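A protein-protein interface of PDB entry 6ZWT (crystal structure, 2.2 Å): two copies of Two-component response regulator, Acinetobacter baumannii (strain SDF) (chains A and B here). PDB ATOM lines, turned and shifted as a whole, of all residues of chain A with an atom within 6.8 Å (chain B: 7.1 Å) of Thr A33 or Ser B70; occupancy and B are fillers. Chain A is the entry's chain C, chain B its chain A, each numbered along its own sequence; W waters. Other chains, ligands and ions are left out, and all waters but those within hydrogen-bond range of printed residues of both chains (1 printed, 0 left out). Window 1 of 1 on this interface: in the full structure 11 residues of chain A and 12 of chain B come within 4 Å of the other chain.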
ATOM      1  N   THR A  30     -10.668  21.219  -8.245  1.00  0.00           N
ATOM      2  CA  THR A  30     -10.131  20.557  -7.038  1.00  0.00           C
ATOM      3  C   THR A  30     -11.190  20.606  -5.937  1.00  0.00           C
ATOM      4  O   THR A  30     -11.648  21.691  -5.619  1.00  0.00           O
ATOM      5  CB  THR A  30      -8.787  21.160  -6.623  1.00  0.00           C
ATOM      6  OG1 THR A  30      -7.801  20.942  -7.639  1.00  0.00           O
ATOM      7  CG2 THR A  30      -8.291  20.550  -5.331  1.00  0.00           C
ATOM      8  N   LEU A  31     -11.597  19.443  -5.441  1.00  0.00           N
ATOM      9  CA  LEU A  31     -12.449  19.286  -4.242  1.00  0.00           C
ATOM     10  C   LEU A  31     -11.631  18.602  -3.142  1.00  0.00           C
ATOM     11  O   LEU A  31     -10.766  17.842  -3.489  1.00  0.00           O
ATOM     12  CB  LEU A  31     -13.661  18.422  -4.611  1.00  0.00           C
ATOM     13  CG  LEU A  31     -14.721  19.033  -5.527  1.00  0.00           C
ATOM     14  CD1 LEU A  31     -15.961  18.164  -5.468  1.00  0.00           C
ATOM     15  CD2 LEU A  31     -15.040  20.492  -5.158  1.00  0.00           C
ATOM     16  N   THR A  32     -11.927  18.821  -1.866  1.00  0.00           N
ATOM     17  CA  THR A  32     -11.388  17.967  -0.776  1.00  0.00           C
ATOM     18  C   THR A  32     -12.129  16.636  -0.818  1.00  0.00           C
ATOM     19  O   THR A  32     -13.219  16.603  -1.416  1.00  0.00           O
ATOM     20  CB  THR A  32     -11.508  18.645   0.595  1.00  0.00           C
ATOM     21  OG1 THR A  32     -12.882  18.782   0.954  1.00  0.00           O
ATOM     22  CG2 THR A  32     -10.803  19.985   0.616  1.00  0.00           C
ATOM     23  N   THR A  33     -11.597  15.595  -0.181  1.00  0.00           N
ATOM     24  CA  THR A  33     -12.296  14.284  -0.082  1.00  0.00           C
ATOM     25  C   THR A  33     -13.675  14.494   0.564  1.00  0.00           C
ATOM     26  O   THR A  33     -14.637  13.830   0.136  1.00  0.00           O
ATOM     27  CB  THR A  33     -11.504  13.241   0.724  1.00  0.00           C
ATOM     28  OG1 THR A  33     -11.302  13.751   2.044  1.00  0.00           O
ATOM     29  CG2 THR A  33     -10.180  12.872   0.090  1.00  0.00           C
ATOM     30  N   GLY A  34     -13.767  15.375   1.558  1.00  0.00           N
ATOM     31  CA  GLY A  34     -15.018  15.607   2.290  1.00  0.00           C
ATOM     32  C   GLY A  34     -16.034  16.313   1.410  1.00  0.00           C
ATOM     33  O   GLY A  34     -17.229  15.920   1.433  1.00  0.00           O
ATOM     34  N   GLU A  35     -15.586  17.342   0.680  1.00  0.00           N
ATOM     35  CA  GLU A  35     -16.453  18.110  -0.246  1.00  0.00           C
ATOM     36  C   GLU A  35     -16.994  17.123  -1.286  1.00  0.00           C
ATOM     37  O   GLU A  35     -18.203  17.193  -1.615  1.00  0.00           O
ATOM     38  CB  GLU A  35     -15.674  19.269  -0.883  1.00  0.00           C
ATOM     39  CG  GLU A  35     -15.395  20.433   0.054  1.00  0.00           C
ATOM     40  CD  GLU A  35     -14.212  21.325  -0.317  1.00  0.00           C
ATOM     41  OE1 GLU A  35     -13.540  21.081  -1.370  1.00  0.00           O
ATOM     42  OE2 GLU A  35     -13.953  22.275   0.463  1.00  0.00           O
ATOM     43  N   PHE A  36     -16.139  16.214  -1.771  1.00  0.00           N
ATOM     44  CA  PHE A  36     -16.525  15.256  -2.839  1.00  0.00           C
ATOM     45  C   PHE A  36     -17.589  14.325  -2.275  1.00  0.00           C
ATOM     46  O   PHE A  36     -18.634  14.088  -2.921  1.00  0.00           O
ATOM     47  CB  PHE A  36     -15.343  14.473  -3.416  1.00  0.00           C
ATOM     48  CG  PHE A  36     -15.808  13.316  -4.261  1.00  0.00           C
ATOM     49  CD1 PHE A  36     -16.252  13.514  -5.568  1.00  0.00           C
ATOM     50  CD2 PHE A  36     -15.916  12.044  -3.711  1.00  0.00           C
ATOM     51  CE1 PHE A  36     -16.783  12.466  -6.309  1.00  0.00           C
ATOM     52  CE2 PHE A  36     -16.421  10.991  -4.461  1.00  0.00           C
ATOM     53  CZ  PHE A  36     -16.854  11.209  -5.757  1.00  0.00           C
ATOM     54  N   ALA A  37     -17.326  13.805  -1.081  1.00  0.00           N
ATOM     55  CA  ALA A  37     -18.190  12.803  -0.419  1.00  0.00           C
ATOM     56  C   ALA A  37     -19.569  13.411  -0.143  1.00  0.00           C
ATOM     57  O   ALA A  37     -20.584  12.726  -0.367  1.00  0.00           O
ATOM     58  CB  ALA A  37     -17.506  12.341   0.826  1.00  0.00           C
ATOM     59  N   VAL A  38     -19.598  14.658   0.333  1.00  0.00           N
ATOM     60  CA  VAL A  38     -20.845  15.398   0.642  1.00  0.00           C
ATOM     61  C   VAL A  38     -21.548  15.699  -0.677  1.00  0.00           C
ATOM     62  O   VAL A  38     -22.748  15.432  -0.777  1.00  0.00           O
ATOM     63  CB  VAL A  38     -20.528  16.653   1.470  1.00  0.00           C
ATOM     64  CG1 VAL A  38     -21.630  17.702   1.437  1.00  0.00           C
ATOM     65  CG2 VAL A  38     -20.232  16.248   2.903  1.00  0.00           C
ATOM     66  N   ALA A  59     -21.602  10.445   3.605  1.00  0.00           N
ATOM     67  CA  ALA A  59     -20.274  10.999   3.257  1.00  0.00           C
ATOM     68  C   ALA A  59     -19.147  10.182   3.911  1.00  0.00           C
ATOM     69  O   ALA A  59     -18.189   9.847   3.195  1.00  0.00           O
ATOM     70  CB  ALA A  59     -20.212  12.456   3.650  1.00  0.00           C
ATOM     71  N   ARG A  60     -19.173   9.947   5.224  1.00  0.00           N
ATOM     72  CA  ARG A  60     -17.925   9.628   5.979  1.00  0.00           C
ATOM     73  C   ARG A  60     -18.099   8.424   6.911  1.00  0.00           C
ATOM     74  O   ARG A  60     -17.074   8.006   7.487  1.00  0.00           O
ATOM     75  CB  ARG A  60     -17.452  10.861   6.763  1.00  0.00           C
ATOM     76  CG  ARG A  60     -16.679  11.886   5.934  1.00  0.00           C
ATOM     77  CD  ARG A  60     -15.173  11.673   5.853  1.00  0.00           C
ATOM     78  NE  ARG A  60     -14.651  12.000   4.524  1.00  0.00           N
ATOM     79  CZ  ARG A  60     -14.315  11.119   3.576  1.00  0.00           C
ATOM     80  NH1 ARG A  60     -14.423   9.817   3.764  1.00  0.00           N
ATOM     81  NH2 ARG A  60     -13.859  11.555   2.423  1.00  0.00           N
ATOM     82  N   GLN A  74     -18.569  22.411   4.991  1.00  0.00           N
ATOM     83  CA  GLN A  74     -18.371  21.700   3.709  1.00  0.00           C
ATOM     84  C   GLN A  74     -19.428  22.156   2.699  1.00  0.00           C
ATOM     85  O   GLN A  74     -19.038  22.530   1.579  1.00  0.00           O
ATOM     86  CB  GLN A  74     -18.423  20.193   3.963  1.00  0.00           C
ATOM     87  CG  GLN A  74     -17.135  19.697   4.565  1.00  0.00           C
ATOM     88  CD  GLN A  74     -17.217  18.253   4.950  1.00  0.00           C
ATOM     89  OE1 GLN A  74     -18.233  17.782   5.422  1.00  0.00           O
ATOM     90  NE2 GLN A  74     -16.103  17.567   4.837  1.00  0.00           N
ATOM     91  N   THR B  33     -13.465  17.188   9.197  1.00  0.00           N
ATOM     92  CA  THR B  33     -12.808  15.882   9.450  1.00  0.00           C
ATOM     93  C   THR B  33     -11.470  15.839   8.710  1.00  0.00           C
ATOM     94  O   THR B  33     -10.513  15.290   9.280  1.00  0.00           O
ATOM     95  CB  THR B  33     -13.688  14.699   9.015  1.00  0.00           C
ATOM     96  OG1 THR B  33     -13.961  14.828   7.618  1.00  0.00           O
ATOM     97  CG2 THR B  33     -14.975  14.591   9.808  1.00  0.00           C
ATOM     98  N   GLY B  34     -11.400  16.367   7.484  1.00  0.00           N
ATOM     99  CA  GLY B  34     -10.180  16.328   6.666  1.00  0.00           C
ATOM    100  C   GLY B  34      -9.107  17.228   7.253  1.00  0.00           C
ATOM    101  O   GLY B  34      -7.917  16.815   7.300  1.00  0.00           O
ATOM    102  N   VAL B  38      -5.512  15.850   8.657  1.00  0.00           N
ATOM    103  CA  VAL B  38      -4.253  16.417   8.115  1.00  0.00           C
ATOM    104  C   VAL B  38      -3.497  17.049   9.287  1.00  0.00           C
ATOM    105  O   VAL B  38      -2.303  16.773   9.446  1.00  0.00           O
ATOM    106  CB  VAL B  38      -4.559  17.419   6.985  1.00  0.00           C
ATOM    107  CG1 VAL B  38      -3.419  18.410   6.722  1.00  0.00           C
ATOM    108  CG2 VAL B  38      -4.955  16.681   5.724  1.00  0.00           C
ATOM    109  N   ARG B  52       3.167  15.328  -0.061  1.00  0.00           N
ATOM    110  CA  ARG B  52       1.711  15.520  -0.200  1.00  0.00           C
ATOM    111  C   ARG B  52       1.023  14.146  -0.208  1.00  0.00           C
ATOM    112  O   ARG B  52      -0.128  14.071   0.294  1.00  0.00           O
ATOM    113  CB  ARG B  52       1.455  16.354  -1.450  1.00  0.00           C
ATOM    114  CG  ARG B  52       0.174  17.154  -1.376  1.00  0.00           C
ATOM    115  CD  ARG B  52      -0.010  18.057  -2.566  1.00  0.00           C
ATOM    116  NE  ARG B  52      -0.205  17.260  -3.758  1.00  0.00           N
ATOM    117  CZ  ARG B  52       0.153  17.630  -4.980  1.00  0.00           C
ATOM    118  NH1 ARG B  52       0.703  18.810  -5.170  1.00  0.00           N
ATOM    119  NH2 ARG B  52      -0.020  16.807  -5.996  1.00  0.00           N
ATOM    120  N   MET B  56      -1.708  12.510   2.580  1.00  0.00           N
ATOM    121  CA  MET B  56      -3.014  11.975   2.120  1.00  0.00           C
ATOM    122  C   MET B  56      -3.133  10.524   2.592  1.00  0.00           C
ATOM    123  O   MET B  56      -4.222  10.147   3.035  1.00  0.00           O
ATOM    124  CB  MET B  56      -3.163  12.073   0.593  1.00  0.00           C
ATOM    125  CG  MET B  56      -4.520  11.646   0.032  1.00  0.00           C
ATOM    126  SD  MET B  56      -5.986  12.480   0.725  1.00  0.00           S
ATOM    127  CE  MET B  56      -6.454  13.529  -0.655  1.00  0.00           C
ATOM    128  N   ARG B  60      -6.208  10.074   5.175  1.00  0.00           N
ATOM    129  CA  ARG B  60      -7.462   9.632   4.505  1.00  0.00           C
ATOM    130  C   ARG B  60      -7.374   8.214   3.945  1.00  0.00           C
ATOM    131  O   ARG B  60      -8.429   7.696   3.610  1.00  0.00           O
ATOM    132  CB  ARG B  60      -7.819  10.633   3.400  1.00  0.00           C
ATOM    133  CG  ARG B  60      -8.598  11.841   3.891  1.00  0.00           C
ATOM    134  CD  ARG B  60     -10.055  11.449   4.103  1.00  0.00           C
ATOM    135  NE  ARG B  60     -10.719  12.292   5.085  1.00  0.00           N
ATOM    136  CZ  ARG B  60     -10.896  12.007   6.375  1.00  0.00           C
ATOM    137  NH1 ARG B  60     -10.449  10.885   6.915  1.00  0.00           N
ATOM    138  NH2 ARG B  60     -11.534  12.868   7.141  1.00  0.00           N
ATOM    139  N   GLY B  61      -6.186   7.607   3.886  1.00  0.00           N
ATOM    140  CA  GLY B  61      -5.958   6.312   3.219  1.00  0.00           C
ATOM    141  C   GLY B  61      -5.536   6.523   1.778  1.00  0.00           C
ATOM    142  O   GLY B  61      -5.675   7.665   1.252  1.00  0.00           O
ATOM    143  N   TRP B  64      -7.697   7.443  -1.754  1.00  0.00           N
ATOM    144  CA  TRP B  64      -8.030   8.858  -2.061  1.00  0.00           C
ATOM    145  C   TRP B  64      -6.843   9.500  -2.743  1.00  0.00           C
ATOM    146  O   TRP B  64      -6.914  10.705  -3.037  1.00  0.00           O
ATOM    147  CB  TRP B  64      -8.423   9.630  -0.798  1.00  0.00           C
ATOM    148  CG  TRP B  64      -9.712   9.147  -0.218  1.00  0.00           C
ATOM    149  CD1 TRP B  64      -9.862   8.263   0.806  1.00  0.00           C
ATOM    150  CD2 TRP B  64     -11.042   9.444  -0.683  1.00  0.00           C
ATOM    151  NE1 TRP B  64     -11.189   8.007   1.033  1.00  0.00           N
ATOM    152  CE2 TRP B  64     -11.937   8.722   0.141  1.00  0.00           C
ATOM    153  CE3 TRP B  64     -11.564  10.260  -1.698  1.00  0.00           C
ATOM    154  CZ2 TRP B  64     -13.318   8.801  -0.009  1.00  0.00           C
ATOM    155  CZ3 TRP B  64     -12.933  10.336  -1.846  1.00  0.00           C
ATOM    156  CH2 TRP B  64     -13.795   9.618  -1.010  1.00  0.00           C
ATOM    157  N   GLY B  65      -5.801   8.710  -2.992  1.00  0.00           N
ATOM    158  CA  GLY B  65      -4.500   9.216  -3.455  1.00  0.00           C
ATOM    159  C   GLY B  65      -4.618  10.065  -4.711  1.00  0.00           C
ATOM    160  O   GLY B  65      -3.737  10.915  -4.952  1.00  0.00           O
ATOM    161  N   ALA B  66      -5.639   9.848  -5.529  1.00  0.00           N
ATOM    162  CA  ALA B  66      -5.789  10.619  -6.790  1.00  0.00           C
ATOM    163  C   ALA B  66      -6.316  12.048  -6.516  1.00  0.00           C
ATOM    164  O   ALA B  66      -6.390  12.811  -7.462  1.00  0.00           O
ATOM    165  CB  ALA B  66      -6.665   9.864  -7.753  1.00  0.00           C
ATOM    166  N   MET B  67      -6.687  12.393  -5.276  1.00  0.00           N
ATOM    167  CA  MET B  67      -7.152  13.754  -4.901  1.00  0.00           C
ATOM    168  C   MET B  67      -6.081  14.465  -4.068  1.00  0.00           C
ATOM    169  O   MET B  67      -6.390  15.474  -3.467  1.00  0.00           O
ATOM    170  CB  MET B  67      -8.458  13.676  -4.113  1.00  0.00           C
ATOM    171  CG  MET B  67      -9.599  13.114  -4.945  1.00  0.00           C
ATOM    172  SD  MET B  67     -11.184  13.276  -4.114  1.00  0.00           S
ATOM    173  CE  MET B  67     -11.971  11.826  -4.803  1.00  0.00           C
ATOM    174  N   GLU B  68      -4.866  13.929  -4.062  1.00  0.00           N
ATOM    175  CA  GLU B  68      -3.610  14.542  -3.551  1.00  0.00           C
ATOM    176  C   GLU B  68      -3.654  16.085  -3.509  1.00  0.00           C
ATOM    177  O   GLU B  68      -3.336  16.582  -2.439  1.00  0.00           O
ATOM    178  CB  GLU B  68      -2.465  14.052  -4.427  1.00  0.00           C
ATOM    179  CG  GLU B  68      -1.186  13.729  -3.689  1.00  0.00           C
ATOM    180  CD  GLU B  68       0.001  14.047  -4.574  1.00  0.00           C
ATOM    181  OE1 GLU B  68      -0.164  13.909  -5.814  1.00  0.00           O
ATOM    182  OE2 GLU B  68       1.050  14.498  -4.038  1.00  0.00           O
ATOM    183  N   ARG B  69      -4.081  16.815  -4.556  1.00  0.00           N
ATOM    184  CA  ARG B  69      -4.040  18.312  -4.571  1.00  0.00           C
ATOM    185  C   ARG B  69      -4.921  18.911  -3.466  1.00  0.00           C
ATOM    186  O   ARG B  69      -4.700  20.077  -3.095  1.00  0.00           O
ATOM    187  CB  ARG B  69      -4.492  18.881  -5.912  1.00  0.00           C
ATOM    188  CG  ARG B  69      -3.579  18.534  -7.071  1.00  0.00           C
ATOM    189  CD  ARG B  69      -3.813  19.416  -8.288  1.00  0.00           C
ATOM    190  NE  ARG B  69      -3.032  18.952  -9.417  1.00  0.00           N
ATOM    191  CZ  ARG B  69      -3.295  17.833 -10.105  1.00  0.00           C
ATOM    192  NH1 ARG B  69      -4.322  17.058  -9.781  1.00  0.00           N
ATOM    193  NH2 ARG B  69      -2.517  17.473 -11.115  1.00  0.00           N
ATOM    194  N   SER B  70      -5.935  18.157  -3.047  1.00  0.00           N
ATOM    195  CA  SER B  70      -6.843  18.405  -1.891  1.00  0.00           C
ATOM    196  C   SER B  70      -6.011  18.883  -0.690  1.00  0.00           C
ATOM    197  O   SER B  70      -6.388  19.831  -0.032  1.00  0.00           O
ATOM    198  CB  SER B  70      -7.628  17.116  -1.607  1.00  0.00           C
ATOM    199  OG  SER B  70      -8.308  17.097  -0.354  1.00  0.00           O
ATOM    200  N   ILE B  71      -4.858  18.271  -0.459  1.00  0.00           N
ATOM    201  CA  ILE B  71      -3.996  18.530   0.737  1.00  0.00           C
ATOM    202  C   ILE B  71      -3.519  19.972   0.762  1.00  0.00           C
ATOM    203  O   ILE B  71      -3.537  20.543   1.827  1.00  0.00           O
ATOM    204  CB  ILE B  71      -2.811  17.558   0.765  1.00  0.00           C
ATOM    205  CG1 ILE B  71      -3.301  16.115   0.847  1.00  0.00           C
ATOM    206  CG2 ILE B  71      -1.895  17.916   1.912  1.00  0.00           C
ATOM    207  CD1 ILE B  71      -3.771  15.689   2.200  1.00  0.00           C
ATOM    208  N   ASP B  72      -3.053  20.510  -0.357  1.00  0.00           N
ATOM    209  CA  ASP B  72      -2.561  21.914  -0.417  1.00  0.00           C
ATOM    210  C   ASP B  72      -3.677  22.867   0.023  1.00  0.00           C
ATOM    211  O   ASP B  72      -3.416  23.817   0.784  1.00  0.00           O
ATOM    212  CB  ASP B  72      -2.047  22.294  -1.805  1.00  0.00           C
ATOM    213  CG  ASP B  72      -0.798  21.557  -2.271  1.00  0.00           C
ATOM    214  OD1 ASP B  72       0.126  21.328  -1.461  1.00  0.00           O
ATOM    215  OD2 ASP B  72      -0.752  21.219  -3.456  1.00  0.00           O
ATOM    216  N   VAL B  73      -4.904  22.612  -0.423  1.00  0.00           N
ATOM    217  CA  VAL B  73      -6.090  23.430  -0.035  1.00  0.00           C
ATOM    218  C   VAL B  73      -6.298  23.313   1.491  1.00  0.00           C
ATOM    219  O   VAL B  73      -6.497  24.356   2.176  1.00  0.00           O
ATOM    220  CB  VAL B  73      -7.328  22.992  -0.830  1.00  0.00           C
ATOM    221  CG1 VAL B  73      -8.564  23.758  -0.393  1.00  0.00           C
ATOM    222  CG2 VAL B  73      -7.097  23.110  -2.341  1.00  0.00           C
ATOM    223  N   GLN B  74      -6.279  22.080   2.000  1.00  0.00           N
ATOM    224  CA  GLN B  74      -6.504  21.758   3.421  1.00  0.00           C
ATOM    225  C   GLN B  74      -5.435  22.428   4.291  1.00  0.00           C
ATOM    226  O   GLN B  74      -5.800  23.100   5.286  1.00  0.00           O
ATOM    227  CB  GLN B  74      -6.534  20.251   3.568  1.00  0.00           C
ATOM    228  CG  GLN B  74      -7.873  19.697   3.120  1.00  0.00           C
ATOM    229  CD  GLN B  74      -7.860  18.196   3.160  1.00  0.00           C
ATOM    230  OE1 GLN B  74      -6.862  17.589   2.816  1.00  0.00           O
ATOM    231  NE2 GLN B  74      -8.971  17.605   3.589  1.00  0.00           N
ATOM    232  N   VAL B  75      -4.162  22.312   3.902  1.00  0.00           N
ATOM    233  CA  VAL B  75      -3.060  23.019   4.616  1.00  0.00           C
ATOM    234  C   VAL B  75      -3.318  24.532   4.587  1.00  0.00           C
ATOM    235  O   VAL B  75      -3.139  25.189   5.626  1.00  0.00           O
ATOM    236  CB  VAL B  75      -1.690  22.692   4.006  1.00  0.00           C
ATOM    237  CG1 VAL B  75      -0.626  23.639   4.530  1.00  0.00           C
ATOM    238  CG2 VAL B  75      -1.330  21.245   4.274  1.00  0.00           C
ATOM    239  N   SER B  76      -3.669  25.105   3.446  1.00  0.00           N
ATOM    240  CA  SER B  76      -3.818  26.579   3.394  1.00  0.00           C
ATOM    241  C   SER B  76      -4.973  26.997   4.338  1.00  0.00           C
ATOM    242  O   SER B  76      -4.877  28.078   4.931  1.00  0.00           O
ATOM    243  CB  SER B  76      -3.918  27.079   1.949  1.00  0.00           C
ATOM    244  OG  SER B  76      -5.242  26.962   1.470  1.00  0.00           O
ATOM    245  N   ARG B  77      -5.991  26.158   4.557  1.00  0.00           N
ATOM    246  CA  ARG B  77      -7.131  26.503   5.458  1.00  0.00           C
ATOM    247  C   ARG B  77      -6.687  26.399   6.932  1.00  0.00           C
ATOM    248  O   ARG B  77      -7.019  27.298   7.746  1.00  0.00           O
ATOM    249  CB  ARG B  77      -8.333  25.603   5.168  1.00  0.00           C
ATOM    250  CG  ARG B  77      -9.075  25.990   3.901  1.00  0.00           C
ATOM    251  CD  ARG B  77      -9.884  24.847   3.345  1.00  0.00           C
ATOM    252  NE  ARG B  77     -10.705  25.323   2.253  1.00  0.00           N
ATOM    253  CZ  ARG B  77     -11.478  24.567   1.479  1.00  0.00           C
ATOM    254  NH1 ARG B  77     -11.557  23.261   1.679  1.00  0.00           N
ATOM    255  NH2 ARG B  77     -12.173  25.137   0.503  1.00  0.00           N
HETATM  256  O   HOH W   1     -14.141  21.610   3.255  1.00  0.00           O
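Among the printed residues, merely in contact across the chains: Leu A31 with Ser B70, Thr A32 with Ser B70, Thr A32 with Gln B74, Thr A32 with Arg B77, Thr A33 with Met B56, Thr A33 with Trp B64, Thr A33 with Ser B70, Phe A36 with Trp B64, Arg A60 with Thr B33, Arg A60 with Arg B60 and Arg A60 with Trp B64.
Thr A33 touches Arg B60, and with the chains exchanged Arg A60 touches Thr B33.
Arg A60 touches its own counterpart, Arg B60.
Positions printed for both chains: 33, 34, 38, 60 and 74.
Water W1 lies within hydrogen-bond range of the side-chain carboxylate of Glu A35 (2.9 Å) and the guanidinium group of Arg B77 (3.4 Å).
OG1 of Thr B33 sits at hydrogen-bond distance from NH2 of Arg B60 (3.2 Å).
O of Met B56 is in hydrogen-bond range of N of Gly B61 (3.3 Å).
NH2 of Arg A60 lies within hydrogen-bond range of O of Thr A33 (3.3 Å).
N of Thr A32 is in hydrogen-bond range of OE1 of Glu A35 (2.8 Å).
Printed residues of chain B within 4 Å of Leu A31: Ser B70.
Thr A33 touches four residues of chain B.
Of the printed residues of chain B, Phe A36 touches Trp B64.
Of the printed residues of chain A, Thr B33 touches Arg A60.
Printed residues of chain A within 4 Å of Met B56: Thr A33.
Printed residues of chain A within 4 Å of Gln B74: Thr A32.
The side-chain hydroxyl (OG1) of Thr A33 lies close to the guanidinium group (NE) of Arg B60 (3.4 Å).
The guanidinium group (NH1) of Arg B77 lies within salt-bridge range of the side-chain carboxylate (OE2) of Glu A35.
Of the 12 printed residues of chain A, 6 touch a printed residue of chain B.
Hydrophobic or aromatic side chains of chain A that line the printed part of chain B: Phe A36.
Of the 21 printed residues of chain B, 7 touch a printed residue of chain A.
Printed residues of chain B that touch a printed residue of chain A: Thr B33, Met B56, Arg B60, Trp B64, Ser B70, Gln B74 and Arg B77.
Hydrophobic or aromatic side chains of chain B within 4 Å of the printed part of chain A: Met B56 and Trp B64.
Along chain B the printed residues that touch a printed residue of chain A span positions 33 to 77.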
